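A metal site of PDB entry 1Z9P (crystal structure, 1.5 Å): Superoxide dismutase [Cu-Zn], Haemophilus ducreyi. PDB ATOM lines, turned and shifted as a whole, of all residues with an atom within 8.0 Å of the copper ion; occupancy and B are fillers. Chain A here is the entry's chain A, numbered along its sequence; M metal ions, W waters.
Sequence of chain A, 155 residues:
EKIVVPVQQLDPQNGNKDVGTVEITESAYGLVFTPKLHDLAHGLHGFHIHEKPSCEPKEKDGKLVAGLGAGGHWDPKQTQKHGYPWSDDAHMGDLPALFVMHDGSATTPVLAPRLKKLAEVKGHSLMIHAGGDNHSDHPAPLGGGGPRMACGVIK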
ATOM      1  N   GLY A  46     -23.241 -16.357  33.072  1.00  0.00           N
ATOM      2  CA  GLY A  46     -22.788 -15.501  31.939  1.00  0.00           C
ATOM      3  C   GLY A  46     -22.630 -14.052  32.395  1.00  0.00           C
ATOM      4  O   GLY A  46     -23.429 -13.558  33.197  1.00  0.00           O
ATOM      5  N   PHE A  47     -21.517 -13.428  31.986  1.00  0.00           N
ATOM      6  CA  PHE A  47     -21.107 -12.138  32.489  1.00  0.00           C
ATOM      7  C   PHE A  47     -20.578 -11.367  31.268  1.00  0.00           C
ATOM      8  O   PHE A  47     -19.582 -11.729  30.664  1.00  0.00           O
ATOM      9  CB  PHE A  47     -20.058 -12.396  33.531  1.00  0.00           C
ATOM     10  CG  PHE A  47     -19.513 -11.165  34.272  1.00  0.00           C
ATOM     11  CD1 PHE A  47     -20.351 -10.167  34.770  1.00  0.00           C
ATOM     12  CD2 PHE A  47     -18.204 -11.127  34.628  1.00  0.00           C
ATOM     13  CE1 PHE A  47     -19.807  -9.108  35.525  1.00  0.00           C
ATOM     14  CE2 PHE A  47     -17.652 -10.095  35.373  1.00  0.00           C
ATOM     15  CZ  PHE A  47     -18.484  -9.087  35.831  1.00  0.00           C
ATOM     16  N   HIS A  48     -21.337 -10.345  30.884  1.00  0.00           N
ATOM     17  CA  HIS A  48     -21.008  -9.588  29.672  1.00  0.00           C
ATOM     18  C   HIS A  48     -21.236  -8.091  29.812  1.00  0.00           C
ATOM     19  O   HIS A  48     -22.080  -7.651  30.570  1.00  0.00           O
ATOM     20  CB  HIS A  48     -21.750 -10.069  28.409  1.00  0.00           C
ATOM     21  CG  HIS A  48     -22.162 -11.509  28.438  1.00  0.00           C
ATOM     22  ND1 HIS A  48     -23.472 -11.891  28.615  1.00  0.00           N
ATOM     23  CD2 HIS A  48     -21.429 -12.641  28.283  1.00  0.00           C
ATOM     24  CE1 HIS A  48     -23.528 -13.221  28.599  1.00  0.00           C
ATOM     25  NE2 HIS A  48     -22.319 -13.696  28.397  1.00  0.00           N
ATOM     26  N   ILE A  49     -20.493  -7.347  29.005  1.00  0.00           N
ATOM     27  CA  ILE A  49     -20.770  -5.917  28.807  1.00  0.00           C
ATOM     28  C   ILE A  49     -21.731  -5.804  27.643  1.00  0.00           C
ATOM     29  O   ILE A  49     -21.496  -6.384  26.572  1.00  0.00           O
ATOM     30  CB  ILE A  49     -19.495  -5.142  28.541  1.00  0.00           C
ATOM     31  CG1 ILE A  49     -18.515  -5.345  29.703  1.00  0.00           C
ATOM     32  CG2 ILE A  49     -19.821  -3.671  28.394  1.00  0.00           C
ATOM     33  CD1 ILE A  49     -17.200  -4.610  29.502  1.00  0.00           C
ATOM     34  N   HIS A  50     -22.857  -5.142  27.908  1.00  0.00           N
ATOM     35  CA  HIS A  50     -23.885  -4.917  26.881  1.00  0.00           C
ATOM     36  C   HIS A  50     -23.767  -3.473  26.416  1.00  0.00           C
ATOM     37  O   HIS A  50     -23.159  -2.620  27.055  1.00  0.00           O
ATOM     38  CB  HIS A  50     -25.302  -5.226  27.402  1.00  0.00           C
ATOM     39  CG  HIS A  50     -25.603  -6.691  27.525  1.00  0.00           C
ATOM     40  ND1 HIS A  50     -26.702  -7.281  26.942  1.00  0.00           N
ATOM     41  CD2 HIS A  50     -24.943  -7.677  28.166  1.00  0.00           C
ATOM     42  CE1 HIS A  50     -26.714  -8.572  27.248  1.00  0.00           C
ATOM     43  NE2 HIS A  50     -25.644  -8.845  27.952  1.00  0.00           N
ATOM     44  N   ALA A  70     -30.736  -2.784  28.005  1.00  0.00           N
ATOM     45  CA  ALA A  70     -29.319  -2.794  27.816  1.00  0.00           C
ATOM     46  C   ALA A  70     -28.894  -3.106  26.395  1.00  0.00           C
ATOM     47  O   ALA A  70     -27.722  -2.921  26.046  1.00  0.00           O
ATOM     48  CB  ALA A  70     -28.697  -3.822  28.739  1.00  0.00           C
ATOM     49  N   GLY A  71     -29.809  -3.613  25.557  1.00  0.00           N
ATOM     50  CA  GLY A  71     -29.450  -4.054  24.226  1.00  0.00           C
ATOM     51  C   GLY A  71     -28.627  -5.319  24.253  1.00  0.00           C
ATOM     52  O   GLY A  71     -28.576  -6.040  25.270  1.00  0.00           O
ATOM     53  N   GLY A  72     -27.941  -5.576  23.142  1.00  0.00           N
ATOM     54  CA  GLY A  72     -27.159  -6.756  22.958  1.00  0.00           C
ATOM     55  C   GLY A  72     -25.776  -6.605  23.516  1.00  0.00           C
ATOM     56  O   GLY A  72     -25.451  -5.607  24.170  1.00  0.00           O
ATOM     57  N   HIS A  73     -24.964  -7.598  23.257  1.00  0.00           N
ATOM     58  CA  HIS A  73     -23.566  -7.587  23.687  1.00  0.00           C
ATOM     59  C   HIS A  73     -22.804  -6.454  23.004  1.00  0.00           C
ATOM     60  O   HIS A  73     -23.020  -6.121  21.827  1.00  0.00           O
ATOM     61  CB  HIS A  73     -22.920  -8.911  23.424  1.00  0.00           C
ATOM     62  CG  HIS A  73     -23.494 -10.025  24.245  1.00  0.00           C
ATOM     63  ND1 HIS A  73     -22.863 -11.232  24.409  1.00  0.00           N
ATOM     64  CD2 HIS A  73     -24.628 -10.105  24.985  1.00  0.00           C
ATOM     65  CE1 HIS A  73     -23.594 -12.027  25.162  1.00  0.00           C
ATOM     66  NE2 HIS A  73     -24.670 -11.364  25.532  1.00  0.00           N
ATOM     67  N   TRP A  74     -21.913  -5.847  23.757  1.00  0.00           N
ATOM     68  CA  TRP A  74     -21.165  -4.720  23.285  1.00  0.00           C
ATOM     69  C   TRP A  74     -20.223  -5.250  22.210  1.00  0.00           C
ATOM     70  O   TRP A  74     -19.434  -6.130  22.438  1.00  0.00           O
ATOM     71  CB  TRP A  74     -20.376  -4.084  24.421  1.00  0.00           C
ATOM     72  CG  TRP A  74     -19.481  -2.941  24.039  1.00  0.00           C
ATOM     73  CD1 TRP A  74     -19.732  -1.864  23.166  1.00  0.00           C
ATOM     74  CD2 TRP A  74     -18.171  -2.731  24.511  1.00  0.00           C
ATOM     75  NE1 TRP A  74     -18.651  -1.035  23.123  1.00  0.00           N
ATOM     76  CE2 TRP A  74     -17.664  -1.533  23.932  1.00  0.00           C
ATOM     77  CE3 TRP A  74     -17.340  -3.434  25.409  1.00  0.00           C
ATOM     78  CZ2 TRP A  74     -16.403  -1.062  24.219  1.00  0.00           C
ATOM     79  CZ3 TRP A  74     -16.083  -2.956  25.686  1.00  0.00           C
ATOM     80  CH2 TRP A  74     -15.625  -1.771  25.097  1.00  0.00           C
ATOM     81  N   HIS A  82     -20.803 -14.229  19.436  1.00  0.00           N
ATOM     82  CA  HIS A  82     -20.473 -14.424  20.844  1.00  0.00           C
ATOM     83  C   HIS A  82     -19.366 -15.451  20.930  1.00  0.00           C
ATOM     84  O   HIS A  82     -19.384 -16.481  20.229  1.00  0.00           O
ATOM     85  CB  HIS A  82     -21.690 -14.932  21.613  1.00  0.00           C
ATOM     86  CG  HIS A  82     -21.445 -15.084  23.069  1.00  0.00           C
ATOM     87  ND1 HIS A  82     -21.286 -13.983  23.896  1.00  0.00           N
ATOM     88  CD2 HIS A  82     -21.277 -16.176  23.864  1.00  0.00           C
ATOM     89  CE1 HIS A  82     -21.050 -14.403  25.125  1.00  0.00           C
ATOM     90  NE2 HIS A  82     -21.018 -15.715  25.134  1.00  0.00           N
ATOM     91  N   HIS A  91     -17.499 -10.813  20.624  1.00  0.00           N
ATOM     92  CA  HIS A  91     -17.935  -9.476  21.066  1.00  0.00           C
ATOM     93  C   HIS A  91     -16.898  -8.961  22.058  1.00  0.00           C
ATOM     94  O   HIS A  91     -16.424  -9.706  22.923  1.00  0.00           O
ATOM     95  CB  HIS A  91     -19.253  -9.497  21.828  1.00  0.00           C
ATOM     96  CG  HIS A  91     -20.372 -10.138  21.081  1.00  0.00           C
ATOM     97  ND1 HIS A  91     -21.180 -11.098  21.635  1.00  0.00           N
ATOM     98  CD2 HIS A  91     -20.843  -9.915  19.827  1.00  0.00           C
ATOM     99  CE1 HIS A  91     -22.100 -11.467  20.747  1.00  0.00           C
ATOM    100  NE2 HIS A  91     -21.918 -10.751  19.646  1.00  0.00           N
ATOM    101  N   GLY A  93     -17.517  -7.265  24.493  1.00  0.00           N
ATOM    102  CA  GLY A  93     -18.146  -7.405  25.830  1.00  0.00           C
ATOM    103  C   GLY A  93     -18.091  -8.776  26.455  1.00  0.00           C
ATOM    104  O   GLY A  93     -18.632  -8.957  27.563  1.00  0.00           O
ATOM    105  N   ASP A  94     -17.497  -9.743  25.791  1.00  0.00           N
ATOM    106  CA  ASP A  94     -17.544 -11.130  26.311  1.00  0.00           C
ATOM    107  C   ASP A  94     -16.481 -11.353  27.405  1.00  0.00           C
ATOM    108  O   ASP A  94     -15.311 -11.415  27.137  1.00  0.00           O
ATOM    109  CB  ASP A  94     -17.355 -12.166  25.205  1.00  0.00           C
ATOM    110  CG  ASP A  94     -18.509 -12.163  24.256  1.00  0.00           C
ATOM    111  OD1 ASP A  94     -19.558 -11.544  24.588  1.00  0.00           O
ATOM    112  OD2 ASP A  94     -18.429 -12.756  23.134  1.00  0.00           O
ATOM    113  N   SER A 125     -23.266  -1.253  29.898  1.00  0.00           N
ATOM    114  CA  SER A 125     -23.871  -1.937  31.034  1.00  0.00           C
ATOM    115  C   SER A 125     -23.136  -3.262  31.279  1.00  0.00           C
ATOM    116  O   SER A 125     -22.575  -3.856  30.374  1.00  0.00           O
ATOM    117  CB  SER A 125     -25.364  -2.166  30.813  1.00  0.00           C
ATOM    118  OG  SER A 125     -25.642  -2.657  29.522  1.00  0.00           O
ATOM    119  N   LEU A 126     -23.153  -3.656  32.543  1.00  0.00           N
ATOM    120  CA  LEU A 126     -22.508  -4.898  33.010  1.00  0.00           C
ATOM    121  C   LEU A 126     -23.623  -5.837  33.406  1.00  0.00           C
ATOM    122  O   LEU A 126     -24.374  -5.550  34.322  1.00  0.00           O
ATOM    123  CB  LEU A 126     -21.612  -4.608  34.215  1.00  0.00           C
ATOM    124  CG  LEU A 126     -20.724  -5.760  34.699  1.00  0.00           C
ATOM    125  CD1 LEU A 126     -19.779  -6.231  33.600  1.00  0.00           C
ATOM    126  CD2 LEU A 126     -19.959  -5.288  35.906  1.00  0.00           C
ATOM    127  N   MET A 127     -23.694  -7.012  32.744  1.00  0.00           N
ATOM    128  CA  MET A 127     -24.828  -7.918  32.888  1.00  0.00           C
ATOM    129  C   MET A 127     -24.355  -9.276  33.439  1.00  0.00           C
ATOM    130  O   MET A 127     -23.334  -9.837  33.005  1.00  0.00           O
ATOM    131  CB  MET A 127     -25.449  -8.152  31.494  1.00  0.00           C
ATOM    132  CG  MET A 127     -26.831  -8.712  31.462  1.00  0.00           C
ATOM    133  SD  MET A 127     -28.096  -7.588  32.090  1.00  0.00           S
ATOM    134  CE  MET A 127     -28.190  -6.439  30.705  1.00  0.00           C
ATOM    135  N   ILE A 128     -25.136  -9.789  34.386  1.00  0.00           N
ATOM    136  CA  ILE A 128     -25.008 -11.131  34.934  1.00  0.00           C
ATOM    137  C   ILE A 128     -26.268 -11.907  34.603  1.00  0.00           C
ATOM    138  O   ILE A 128     -27.397 -11.505  34.913  1.00  0.00           O
ATOM    139  CB  ILE A 128     -24.785 -11.075  36.458  1.00  0.00           C
ATOM    140  CG1 ILE A 128     -23.674 -10.077  36.788  1.00  0.00           C
ATOM    141  CG2 ILE A 128     -24.496 -12.470  36.944  1.00  0.00           C
ATOM    142  CD1 ILE A 128     -23.425  -9.835  38.246  1.00  0.00           C
ATOM    143  N   HIS A 129     -26.098 -13.049  33.941  1.00  0.00           N
ATOM    144  CA  HIS A 129     -27.231 -13.837  33.506  1.00  0.00           C
ATOM    145  C   HIS A 129     -27.587 -14.985  34.482  1.00  0.00           C
ATOM    146  O   HIS A 129     -26.817 -15.365  35.318  1.00  0.00           O
ATOM    147  CB  HIS A 129     -26.958 -14.437  32.113  1.00  0.00           C
ATOM    148  CG  HIS A 129     -26.901 -13.383  31.033  1.00  0.00           C
ATOM    149  ND1 HIS A 129     -27.951 -13.142  30.172  1.00  0.00           N
ATOM    150  CD2 HIS A 129     -25.927 -12.503  30.685  1.00  0.00           C
ATOM    151  CE1 HIS A 129     -27.628 -12.137  29.362  1.00  0.00           C
ATOM    152  NE2 HIS A 129     -26.393 -11.747  29.641  1.00  0.00           N
ATOM    153  N   ASP A 133     -22.250 -19.764  30.453  1.00  0.00           N
ATOM    154  CA  ASP A 133     -21.738 -19.230  29.211  1.00  0.00           C
ATOM    155  C   ASP A 133     -20.784 -20.248  28.583  1.00  0.00           C
ATOM    156  O   ASP A 133     -19.681 -20.461  29.070  1.00  0.00           O
ATOM    157  CB  ASP A 133     -21.001 -17.874  29.470  1.00  0.00           C
ATOM    158  CG  ASP A 133     -20.744 -17.075  28.213  1.00  0.00           C
ATOM    159  OD1 ASP A 133     -20.856 -17.615  27.078  1.00  0.00           O
ATOM    160  OD2 ASP A 133     -20.393 -15.869  28.275  1.00  0.00           O
ATOM    161  N   LEU A 142     -25.815 -16.523  22.462  1.00  0.00           N
ATOM    162  CA  LEU A 142     -25.181 -15.695  23.485  1.00  0.00           C
ATOM    163  C   LEU A 142     -24.729 -16.582  24.660  1.00  0.00           C
ATOM    164  O   LEU A 142     -24.815 -16.201  25.842  1.00  0.00           O
ATOM    165  CB  LEU A 142     -26.098 -14.546  23.904  1.00  0.00           C
ATOM    166  CG  LEU A 142     -26.519 -13.620  22.735  1.00  0.00           C
ATOM    167  CD1 LEU A 142     -27.646 -12.753  23.172  1.00  0.00           C
ATOM    168  CD2 LEU A 142     -25.390 -12.727  22.167  1.00  0.00           C
ATOM    169  N   GLY A 145     -26.755 -17.776  28.295  1.00  0.00           N
ATOM    170  CA  GLY A 145     -26.996 -16.959  29.465  1.00  0.00           C
ATOM    171  C   GLY A 145     -28.489 -16.875  29.806  1.00  0.00           C
ATOM    172  O   GLY A 145     -28.858 -16.856  30.980  1.00  0.00           O
ATOM    173  N   GLY A 146     -29.335 -16.818  28.777  1.00  0.00           N
ATOM    174  CA  GLY A 146     -30.770 -16.693  29.037  1.00  0.00           C
ATOM    175  C   GLY A 146     -31.101 -15.405  29.750  1.00  0.00           C
ATOM    176  O   GLY A 146     -30.481 -14.350  29.468  1.00  0.00           O
ATOM    177  N   PRO A 147     -32.043 -15.469  30.695  1.00  0.00           N
ATOM    178  CA  PRO A 147     -32.515 -14.263  31.345  1.00  0.00           C
ATOM    179  C   PRO A 147     -31.409 -13.433  31.990  1.00  0.00           C
ATOM    180  O   PRO A 147     -30.401 -13.944  32.461  1.00  0.00           O
ATOM    181  CB  PRO A 147     -33.460 -14.791  32.400  1.00  0.00           C
ATOM    182  CG  PRO A 147     -33.982 -16.027  31.796  1.00  0.00           C
ATOM    183  CD  PRO A 147     -32.759 -16.655  31.163  1.00  0.00           C
ATOM    184  N   ARG A 148     -31.693 -12.137  32.022  1.00  0.00           N
ATOM    185  CA  ARG A 148     -30.847 -11.149  32.638  1.00  0.00           C
ATOM    186  C   ARG A 148     -31.214 -11.024  34.104  1.00  0.00           C
ATOM    187  O   ARG A 148     -32.337 -10.565  34.423  1.00  0.00           O
ATOM    188  CB  ARG A 148     -31.065  -9.851  31.867  1.00  0.00           C
ATOM    189  CG  ARG A 148     -30.576  -9.973  30.404  1.00  0.00           C
ATOM    190  CD  ARG A 148     -30.939  -8.852  29.494  1.00  0.00           C
ATOM    191  NE  ARG A 148     -30.600  -9.208  28.110  1.00  0.00           N
ATOM    192  CZ  ARG A 148     -30.293  -8.339  27.149  1.00  0.00           C
ATOM    193  NH1 ARG A 148     -30.264  -7.046  27.377  1.00  0.00           N
ATOM    194  NH2 ARG A 148     -29.939  -8.774  25.946  1.00  0.00           N
ATOM    195  N   ALA A 150     -29.019  -9.799  36.900  1.00  0.00           N
ATOM    196  CA  ALA A 150     -28.486  -8.637  37.576  1.00  0.00           C
ATOM    197  C   ALA A 150     -27.686  -7.770  36.610  1.00  0.00           C
ATOM    198  O   ALA A 150     -27.168  -8.219  35.575  1.00  0.00           O
ATOM    199  CB  ALA A 150     -27.668  -9.047  38.706  1.00  0.00           C
HETATM  200 CU    CU M   1     -25.076 -10.662  28.521  1.00  0.00          CU
HETATM  201 ZN    ZN M   2     -21.181 -11.945  23.513  1.00  0.00          ZN
HETATM  202  O   HOH W   1     -27.375 -11.722  26.360  1.00  0.00           O
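The backbone carbonyl oxygen (O) of Gly 72 lies close to a ring nitrogen (ND1) of His 50 (3.5 Å).
A ring nitrogen (ND1) of His 50 is in hydrogen-bond range of the backbone carbonyl oxygen (O) of Gly 71, 2.8 Å away.
The backbone NH of His 50 sits at hydrogen-bond distance from the backbone carbonyl oxygen of Ser 125, at 2.8 Å.
A ring nitrogen (NE2) of His 73 sits close to a ring nitrogen (ND1) of His 48 (3.3 Å).
A ring nitrogen (NE2) of His 48 lies within hydrogen-bond range of the side-chain carboxylate (OD2) of Asp 133 (2.9 Å).
The backbone NH of His 129 lies within hydrogen-bond range of the backbone carbonyl oxygen of Gly 46.
ND1 of His 129 is in hydrogen-bond range of O of Gly 146, at 2.9 Å.
The backbone carbonyl oxygen (O) of Pro 147 sits close to a ring nitrogen (ND1) of His 129 (3.4 Å).
His 73 touches the copper ion.
Met 127 touches the copper ion (CB to CU, 3.9 Å).
Five residues have an atom within 4 Å of the copper ion: His 48, His 50, His 73, Met 127 and His 129.
Along chain A the residues within 4 Å of the copper ion span positions 48 to 129.
The copper ion is bound by a ring nitrogen (NE2) of His 50 (2.0 Å), a ring nitrogen (ND1) of His 48 (2.0 Å) and a ring nitrogen (NE2) of His 129 (2.0 Å).
The copper ion has three donor atoms within binding distance.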
